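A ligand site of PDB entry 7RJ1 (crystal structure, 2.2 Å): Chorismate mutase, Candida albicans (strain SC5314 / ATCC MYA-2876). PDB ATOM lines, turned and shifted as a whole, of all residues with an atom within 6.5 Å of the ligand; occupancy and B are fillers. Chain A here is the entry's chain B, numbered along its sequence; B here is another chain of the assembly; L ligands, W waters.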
ATOM      1  N   PHE A  37     -11.119  -2.815  13.796  1.00  0.00           N
ATOM      2  CA  PHE A  37     -12.003  -1.677  13.626  1.00  0.00           C
ATOM      3  C   PHE A  37     -12.254  -0.986  14.959  1.00  0.00           C
ATOM      4  O   PHE A  37     -12.048  -1.556  16.034  1.00  0.00           O
ATOM      5  CB  PHE A  37     -13.323  -2.117  12.982  1.00  0.00           C
ATOM      6  CG  PHE A  37     -13.130  -2.898  11.705  1.00  0.00           C
ATOM      7  CD1 PHE A  37     -12.806  -2.247  10.522  1.00  0.00           C
ATOM      8  CD2 PHE A  37     -13.246  -4.286  11.699  1.00  0.00           C
ATOM      9  CE1 PHE A  37     -12.609  -2.964   9.351  1.00  0.00           C
ATOM     10  CE2 PHE A  37     -13.050  -5.003  10.528  1.00  0.00           C
ATOM     11  CZ  PHE A  37     -12.731  -4.342   9.354  1.00  0.00           C
ATOM     12  N   GLN A 135     -16.306   5.368  12.480  1.00  0.00           N
ATOM     13  CA  GLN A 135     -15.701   5.442  11.148  1.00  0.00           C
ATOM     14  C   GLN A 135     -16.784   5.009  10.169  1.00  0.00           C
ATOM     15  O   GLN A 135     -17.072   3.812  10.033  1.00  0.00           O
ATOM     16  CB  GLN A 135     -14.464   4.546  11.042  1.00  0.00           C
ATOM     17  CG  GLN A 135     -13.373   5.095  10.170  1.00  0.00           C
ATOM     18  CD  GLN A 135     -12.045   4.393  10.389  1.00  0.00           C
ATOM     19  OE1 GLN A 135     -10.978   4.984  10.190  1.00  0.00           O
ATOM     20  NE2 GLN A 135     -12.098   3.128  10.789  1.00  0.00           N
ATOM     21  N   LYS A 136     -17.406   5.991   9.510  1.00  0.00           N
ATOM     22  CA  LYS A 136     -18.611   5.718   8.722  1.00  0.00           C
ATOM     23  C   LYS A 136     -18.330   4.711   7.610  1.00  0.00           C
ATOM     24  O   LYS A 136     -19.193   3.868   7.292  1.00  0.00           O
ATOM     25  CB  LYS A 136     -19.175   7.014   8.146  1.00  0.00           C
ATOM     26  CG  LYS A 136     -18.227   7.753   7.201  1.00  0.00           C
ATOM     27  CD  LYS A 136     -18.890   8.990   6.607  1.00  0.00           C
ATOM     28  CE  LYS A 136     -18.129   9.497   5.391  1.00  0.00           C
ATOM     29  NZ  LYS A 136     -18.985  10.309   4.499  1.00  0.00           N
ATOM     30  N   GLU A 137     -17.150   4.760   7.003  1.00  0.00           N
ATOM     31  CA  GLU A 137     -16.817   3.879   5.896  1.00  0.00           C
ATOM     32  C   GLU A 137     -16.504   2.458   6.350  1.00  0.00           C
ATOM     33  O   GLU A 137     -16.123   1.636   5.511  1.00  0.00           O
ATOM     34  CB  GLU A 137     -15.637   4.448   5.111  1.00  0.00           C
ATOM     35  CG  GLU A 137     -14.296   4.303   5.810  1.00  0.00           C
ATOM     36  CD  GLU A 137     -13.994   5.478   6.735  1.00  0.00           C
ATOM     37  OE1 GLU A 137     -14.945   6.169   7.157  1.00  0.00           O
ATOM     38  OE2 GLU A 137     -12.794   5.705   7.029  1.00  0.00           O
ATOM     39  N   ASN A 138     -16.641   2.150   7.640  1.00  0.00           N
ATOM     40  CA  ASN A 138     -16.449   0.781   8.115  1.00  0.00           C
ATOM     41  C   ASN A 138     -17.660   0.316   8.929  1.00  0.00           C
ATOM     42  O   ASN A 138     -17.525  -0.624   9.719  1.00  0.00           O
ATOM     43  CB  ASN A 138     -15.167   0.666   8.937  1.00  0.00           C
ATOM     44  CG  ASN A 138     -13.934   0.528   8.062  1.00  0.00           C
ATOM     45  OD1 ASN A 138     -13.995  -0.057   6.983  1.00  0.00           O
ATOM     46  ND2 ASN A 138     -12.812   1.062   8.525  1.00  0.00           N
ATOM     47  N   LEU A 139     -18.810   0.955   8.762  1.00  0.00           N
ATOM     48  CA  LEU A 139     -20.027   0.469   9.398  1.00  0.00           C
ATOM     49  C   LEU A 139     -20.336  -0.954   8.963  1.00  0.00           C
ATOM     50  O   LEU A 139     -20.669  -1.809   9.796  1.00  0.00           O
ATOM     51  CB  LEU A 139     -21.200   1.394   9.070  1.00  0.00           C
ATOM     52  CG  LEU A 139     -22.590   0.967   9.558  1.00  0.00           C
ATOM     53  CD1 LEU A 139     -22.916   1.621  10.890  1.00  0.00           C
ATOM     54  CD2 LEU A 139     -23.657   1.300   8.527  1.00  0.00           C
ATOM     55  N   GLY A 140     -20.224  -1.235   7.667  1.00  0.00           N
ATOM     56  CA  GLY A 140     -20.502  -2.578   7.191  1.00  0.00           C
ATOM     57  C   GLY A 140     -19.470  -3.591   7.664  1.00  0.00           C
ATOM     58  O   GLY A 140     -19.816  -4.657   8.173  1.00  0.00           O
ATOM     59  N   SER A 141     -18.191  -3.250   7.513  1.00  0.00           N
ATOM     60  CA  SER A 141     -17.117  -4.169   7.890  1.00  0.00           C
ATOM     61  C   SER A 141     -17.193  -4.532   9.362  1.00  0.00           C
ATOM     62  O   SER A 141     -17.036  -5.696   9.743  1.00  0.00           O
ATOM     63  CB  SER A 141     -15.756  -3.539   7.569  1.00  0.00           C
ATOM     64  OG  SER A 141     -15.613  -3.312   6.185  1.00  0.00           O
ATOM     65  N   ALA A 142     -17.425  -3.535  10.221  1.00  0.00           N
ATOM     66  CA  ALA A 142     -17.467  -3.808  11.654  1.00  0.00           C
ATOM     67  C   ALA A 142     -18.702  -4.617  12.027  1.00  0.00           C
ATOM     68  O   ALA A 142     -18.636  -5.507  12.877  1.00  0.00           O
ATOM     69  CB  ALA A 142     -17.411  -2.502  12.451  1.00  0.00           C
ATOM     70  N   SER A 143     -19.844  -4.312  11.398  1.00  0.00           N
ATOM     71  CA  SER A 143     -21.059  -5.065  11.714  1.00  0.00           C
ATOM     72  C   SER A 143     -20.947  -6.517  11.258  1.00  0.00           C
ATOM     73  O   SER A 143     -21.362  -7.429  11.980  1.00  0.00           O
ATOM     74  CB  SER A 143     -22.274  -4.364  11.092  1.00  0.00           C
ATOM     75  OG  SER A 143     -22.171  -4.250   9.688  1.00  0.00           O
ATOM     76  N   THR A 144     -20.378  -6.756  10.076  1.00  0.00           N
ATOM     77  CA  THR A 144     -20.191  -8.139   9.621  1.00  0.00           C
ATOM     78  C   THR A 144     -19.297  -8.915  10.582  1.00  0.00           C
ATOM     79  O   THR A 144     -19.600 -10.066  10.914  1.00  0.00           O
ATOM     80  CB  THR A 144     -19.621  -8.183   8.208  1.00  0.00           C
ATOM     81  OG1 THR A 144     -18.293  -7.662   8.208  1.00  0.00           O
ATOM     82  CG2 THR A 144     -20.498  -7.444   7.219  1.00  0.00           C
ATOM     83  N   HIS B  70     -25.365  -7.161   0.727  1.00  0.00           N
ATOM     84  CA  HIS B  70     -24.303  -6.226   1.097  1.00  0.00           C
ATOM     85  C   HIS B  70     -24.298  -5.006   0.196  1.00  0.00           C
ATOM     86  O   HIS B  70     -23.852  -3.935   0.609  1.00  0.00           O
ATOM     87  CB  HIS B  70     -22.946  -6.926   1.070  1.00  0.00           C
ATOM     88  CG  HIS B  70     -22.689  -7.754   2.297  1.00  0.00           C
ATOM     89  ND1 HIS B  70     -21.562  -8.532   2.446  1.00  0.00           N
ATOM     90  CD2 HIS B  70     -23.422  -7.942   3.422  1.00  0.00           C
ATOM     91  CE1 HIS B  70     -21.607  -9.154   3.619  1.00  0.00           C
ATOM     92  NE2 HIS B  70     -22.730  -8.811   4.226  1.00  0.00           N
ATOM     93  N   ILE B  73     -26.139  -2.036   1.629  1.00  0.00           N
ATOM     94  CA  ILE B  73     -25.506  -1.227   2.660  1.00  0.00           C
ATOM     95  C   ILE B  73     -24.147  -0.749   2.166  1.00  0.00           C
ATOM     96  O   ILE B  73     -23.223  -0.547   2.960  1.00  0.00           O
ATOM     97  CB  ILE B  73     -25.398  -1.990   3.988  1.00  0.00           C
ATOM     98  CG1 ILE B  73     -24.623  -3.295   3.792  1.00  0.00           C
ATOM     99  CG2 ILE B  73     -26.785  -2.286   4.531  1.00  0.00           C
ATOM    100  CD1 ILE B  73     -24.660  -4.196   5.006  1.00  0.00           C
ATOM    101  N   ARG B  74     -24.007  -0.592   0.846  1.00  0.00           N
ATOM    102  CA  ARG B  74     -22.942   0.158   0.176  1.00  0.00           C
ATOM    103  C   ARG B  74     -21.602  -0.569   0.110  1.00  0.00           C
ATOM    104  O   ARG B  74     -20.575   0.089  -0.109  1.00  0.00           O
ATOM    105  CB  ARG B  74     -22.716   1.523   0.833  1.00  0.00           C
ATOM    106  CG  ARG B  74     -23.975   2.351   1.043  1.00  0.00           C
ATOM    107  CD  ARG B  74     -23.703   3.523   1.962  1.00  0.00           C
ATOM    108  NE  ARG B  74     -23.223   3.112   3.276  1.00  0.00           N
ATOM    109  CZ  ARG B  74     -23.259   3.874   4.361  1.00  0.00           C
ATOM    110  NH1 ARG B  74     -23.763   5.097   4.318  1.00  0.00           N
ATOM    111  NH2 ARG B  74     -22.770   3.417   5.501  1.00  0.00           N
ATOM    112  N   ARG B  75     -21.561  -1.898   0.265  1.00  0.00           N
ATOM    113  CA  ARG B  75     -20.284  -2.583   0.317  1.00  0.00           C
ATOM    114  C   ARG B  75     -19.437  -2.311  -0.921  1.00  0.00           C
ATOM    115  O   ARG B  75     -18.208  -2.149  -0.824  1.00  0.00           O
ATOM    116  CB  ARG B  75     -20.484  -4.088   0.481  1.00  0.00           C
ATOM    117  CG  ARG B  75     -19.185  -4.876   0.325  1.00  0.00           C
ATOM    118  CD  ARG B  75     -19.295  -6.304   0.814  1.00  0.00           C
ATOM    119  NE  ARG B  75     -17.984  -6.930   0.894  1.00  0.00           N
ATOM    120  CZ  ARG B  75     -17.696  -7.957   1.690  1.00  0.00           C
ATOM    121  NH1 ARG B  75     -18.606  -8.496   2.471  1.00  0.00           N
ATOM    122  NH2 ARG B  75     -16.456  -8.429   1.694  1.00  0.00           N
ATOM    123  N   TYR B  76     -20.064  -2.222  -2.084  1.00  0.00           N
ATOM    124  CA  TYR B  76     -19.308  -2.120  -3.331  1.00  0.00           C
ATOM    125  C   TYR B  76     -19.190  -0.692  -3.825  1.00  0.00           C
ATOM    126  O   TYR B  76     -18.685  -0.471  -4.938  1.00  0.00           O
ATOM    127  CB  TYR B  76     -19.932  -3.046  -4.368  1.00  0.00           C
ATOM    128  CG  TYR B  76     -19.961  -4.444  -3.821  1.00  0.00           C
ATOM    129  CD1 TYR B  76     -18.786  -5.157  -3.638  1.00  0.00           C
ATOM    130  CD2 TYR B  76     -21.156  -5.039  -3.408  1.00  0.00           C
ATOM    131  CE1 TYR B  76     -18.784  -6.431  -3.098  1.00  0.00           C
ATOM    132  CE2 TYR B  76     -21.170  -6.320  -2.873  1.00  0.00           C
ATOM    133  CZ  TYR B  76     -19.983  -7.003  -2.725  1.00  0.00           C
ATOM    134  OH  TYR B  76     -19.980  -8.268  -2.182  1.00  0.00           O
ATOM    135  N   GLU B  77     -19.595   0.292  -3.016  1.00  0.00           N
ATOM    136  CA  GLU B  77     -19.113   1.650  -3.204  1.00  0.00           C
ATOM    137  C   GLU B  77     -17.653   1.779  -2.762  1.00  0.00           C
ATOM    138  O   GLU B  77     -16.924   2.640  -3.278  1.00  0.00           O
ATOM    139  CB  GLU B  77     -19.987   2.644  -2.423  1.00  0.00           C
ATOM    140  CG  GLU B  77     -19.541   4.095  -2.542  1.00  0.00           C
ATOM    141  CD  GLU B  77     -20.369   5.066  -1.715  1.00  0.00           C
ATOM    142  OE1 GLU B  77     -21.259   4.625  -0.957  1.00  0.00           O
ATOM    143  OE2 GLU B  77     -20.119   6.288  -1.816  1.00  0.00           O
ATOM    144  N   ALA B  78     -17.212   0.929  -1.842  1.00  0.00           N
ATOM    145  CA  ALA B  78     -15.819   0.973  -1.390  1.00  0.00           C
ATOM    146  C   ALA B  78     -14.874   0.604  -2.539  1.00  0.00           C
ATOM    147  O   ALA B  78     -15.140  -0.341  -3.295  1.00  0.00           O
ATOM    148  CB  ALA B  78     -15.602   0.011  -0.220  1.00  0.00           C
ATOM    149  N   ASP B  80     -12.009  -0.828  -2.336  1.00  0.00           N
ATOM    150  CA  ASP B  80     -11.317  -2.080  -2.074  1.00  0.00           C
ATOM    151  C   ASP B  80     -12.252  -3.278  -2.074  1.00  0.00           C
ATOM    152  O   ASP B  80     -11.871  -4.361  -1.624  1.00  0.00           O
ATOM    153  CB  ASP B  80     -10.575  -2.000  -0.736  1.00  0.00           C
ATOM    154  CG  ASP B  80     -11.504  -1.825   0.447  1.00  0.00           C
ATOM    155  OD1 ASP B  80     -12.647  -1.355   0.238  1.00  0.00           O
ATOM    156  OD2 ASP B  80     -11.108  -2.155   1.581  1.00  0.00           O
ATOM    157  N   GLU B  81     -13.473  -3.120  -2.577  1.00  0.00           N
ATOM    158  CA  GLU B  81     -14.431  -4.221  -2.674  1.00  0.00           C
ATOM    159  C   GLU B  81     -14.814  -4.414  -4.133  1.00  0.00           C
ATOM    160  O   GLU B  81     -15.271  -3.468  -4.787  1.00  0.00           O
ATOM    161  CB  GLU B  81     -15.683  -3.933  -1.824  1.00  0.00           C
ATOM    162  CG  GLU B  81     -15.430  -3.831  -0.323  1.00  0.00           C
ATOM    163  CD  GLU B  81     -15.059  -5.168   0.312  1.00  0.00           C
ATOM    164  OE1 GLU B  81     -14.192  -5.177   1.212  1.00  0.00           O
ATOM    165  OE2 GLU B  81     -15.607  -6.207  -0.104  1.00  0.00           O
ATOM    166  N   ILE B  97     -21.539   6.853   0.994  1.00  0.00           N
ATOM    167  CA  ILE B  97     -20.377   7.258   1.794  1.00  0.00           C
ATOM    168  C   ILE B  97     -19.664   8.438   1.142  1.00  0.00           C
ATOM    169  O   ILE B  97     -19.118   9.300   1.838  1.00  0.00           O
ATOM    170  CB  ILE B  97     -19.432   6.057   1.995  1.00  0.00           C
ATOM    171  CG1 ILE B  97     -20.096   5.010   2.883  1.00  0.00           C
ATOM    172  CG2 ILE B  97     -18.080   6.501   2.565  1.00  0.00           C
ATOM    173  CD1 ILE B  97     -20.108   5.390   4.348  1.00  0.00           C
ATOM    174  N   TYR B  99     -16.843   8.480  -1.181  1.00  0.00           N
ATOM    175  CA  TYR B  99     -15.402   8.349  -1.069  1.00  0.00           C
ATOM    176  C   TYR B  99     -14.710   9.389  -1.953  1.00  0.00           C
ATOM    177  O   TYR B  99     -15.212   9.734  -3.028  1.00  0.00           O
ATOM    178  CB  TYR B  99     -14.949   6.957  -1.501  1.00  0.00           C
ATOM    179  CG  TYR B  99     -15.317   5.825  -0.568  1.00  0.00           C
ATOM    180  CD1 TYR B  99     -14.473   5.452   0.465  1.00  0.00           C
ATOM    181  CD2 TYR B  99     -16.493   5.114  -0.752  1.00  0.00           C
ATOM    182  CE1 TYR B  99     -14.795   4.410   1.311  1.00  0.00           C
ATOM    183  CE2 TYR B  99     -16.825   4.062   0.097  1.00  0.00           C
ATOM    184  CZ  TYR B  99     -15.974   3.712   1.122  1.00  0.00           C
ATOM    185  OH  TYR B  99     -16.296   2.670   1.968  1.00  0.00           O
HETATM  186  N1  LIG L   1     -15.650  -0.971   4.572  1.00  0.00           N
HETATM  187  C1  LIG L   1     -16.790  -0.613   3.727  1.00  0.00           C
HETATM  188  C2  LIG L   1     -18.044  -0.398   4.573  1.00  0.00           C
HETATM  189  O1  LIG L   1     -18.999   0.265   4.151  1.00  0.00           O
HETATM  190  C3  LIG L   1     -17.017  -1.674   2.651  1.00  0.00           C
HETATM  191  C4  LIG L   1     -17.287  -3.042   3.193  1.00  0.00           C
HETATM  192  C5  LIG L   1     -16.395  -4.052   3.360  1.00  0.00           C
HETATM  193  C6  LIG L   1     -18.560  -3.566   3.602  1.00  0.00           C
HETATM  194  N2  LIG L   1     -17.016  -5.166   3.867  1.00  0.00           N
HETATM  195  C7  LIG L   1     -18.351  -4.890   4.019  1.00  0.00           C
HETATM  196  C8  LIG L   1     -19.850  -3.029   3.666  1.00  0.00           C
HETATM  197  C9  LIG L   1     -19.391  -5.693   4.487  1.00  0.00           C
HETATM  198  C10 LIG L   1     -20.890  -3.838   4.118  1.00  0.00           C
HETATM  199  C11 LIG L   1     -20.641  -5.150   4.537  1.00  0.00           C
HETATM  200  O2  LIG L   1     -18.144  -0.870   5.709  1.00  0.00           O
HETATM  201  O   HOH W   1     -12.940   0.877   3.632  1.00  0.00           O
HETATM  202  O   HOH W   2     -18.539   1.303   1.662  1.00  0.00           O
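The backbone carbonyl oxygen of Ser 141 is in hydrogen-bond range of the side-chain hydroxyl of Thr 144 (2.8 Å). The backbone carbonyl oxygen (O) of Gly 140 sits close to the side-chain hydroxyl (OG1) of Thr 144. O of Gly 140 is in hydrogen-bond range of OG of Ser 143. The side-chain amide nitrogen (ND2) of Asn 138 sits close to the side-chain amide nitrogen (NE2) of Gln 135 (3.1 Å). OE2 of Glu 81 of chain B lies within salt-bridge range of NE of Arg 75 of chain B, 2.7 Å away. A ring nitrogen (ND1) of His 70 of chain B sits at hydrogen-bond distance from the guanidinium group of Arg 75 of chain B (3.0 Å). OG of Ser 143 is in hydrogen-bond range of O of Leu 139 (2.9 Å).
Water W2 lies within hydrogen-bond range of the side-chain hydroxyl (OH) of Tyr 99 of chain B, an oxygen (O1) of the ligand and the backbone carbonyl oxygen (O) of Arg 74 of chain B.
N of Leu 139 touches O2 of the ligand, 3.6 Å away. CG2 of Thr 144 touches C9 of the ligand (3.4 Å). His 70 of chain B touches the ligand (CG to C11, 3.999 Å). Ile 73 of chain B touches the ligand (CG1 to C10, 3.8 Å). Arg 75 of chain B touches the ligand. CB of Ala 78 of chain B touches C3 of the ligand, at 3.6 Å. OE1 of Glu 81 of chain B touches C5 of the ligand, 3.3 Å away. OH of Tyr 99 of chain B touches C1 of the ligand, 3.8 Å away. Hydrophobic or aromatic side chains within 4 Å of the ligand: His 70 of chain B, Ile 73 of chain B and Ala 78 of chain B. Within 4 Å of the ligand: Glu 137, Asn 138, Leu 139, Gly 140, Ser 141, Thr 144, His 70 of chain B, Ile 73 of chain B, Arg 75 of chain B, Ala 78 of chain B, Glu 81 of chain B and Tyr 99 of chain B. Along chain A the residues within 4 Å of the ligand span positions 137 to 144.
O of Glu 137 is in hydrogen-bond range of N1 of the ligand (2.8 Å). The backbone NH (N) of Ser 141 lies within hydrogen-bond range of an oxygen (O2) of the ligand. OG of Ser 141 is in hydrogen-bond range of N1 of the ligand (2.8 Å). N of Gly 140 is in hydrogen-bond range of O2 of the ligand. OD1 of Asn 138 lies within hydrogen-bond range of N1 of the ligand.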
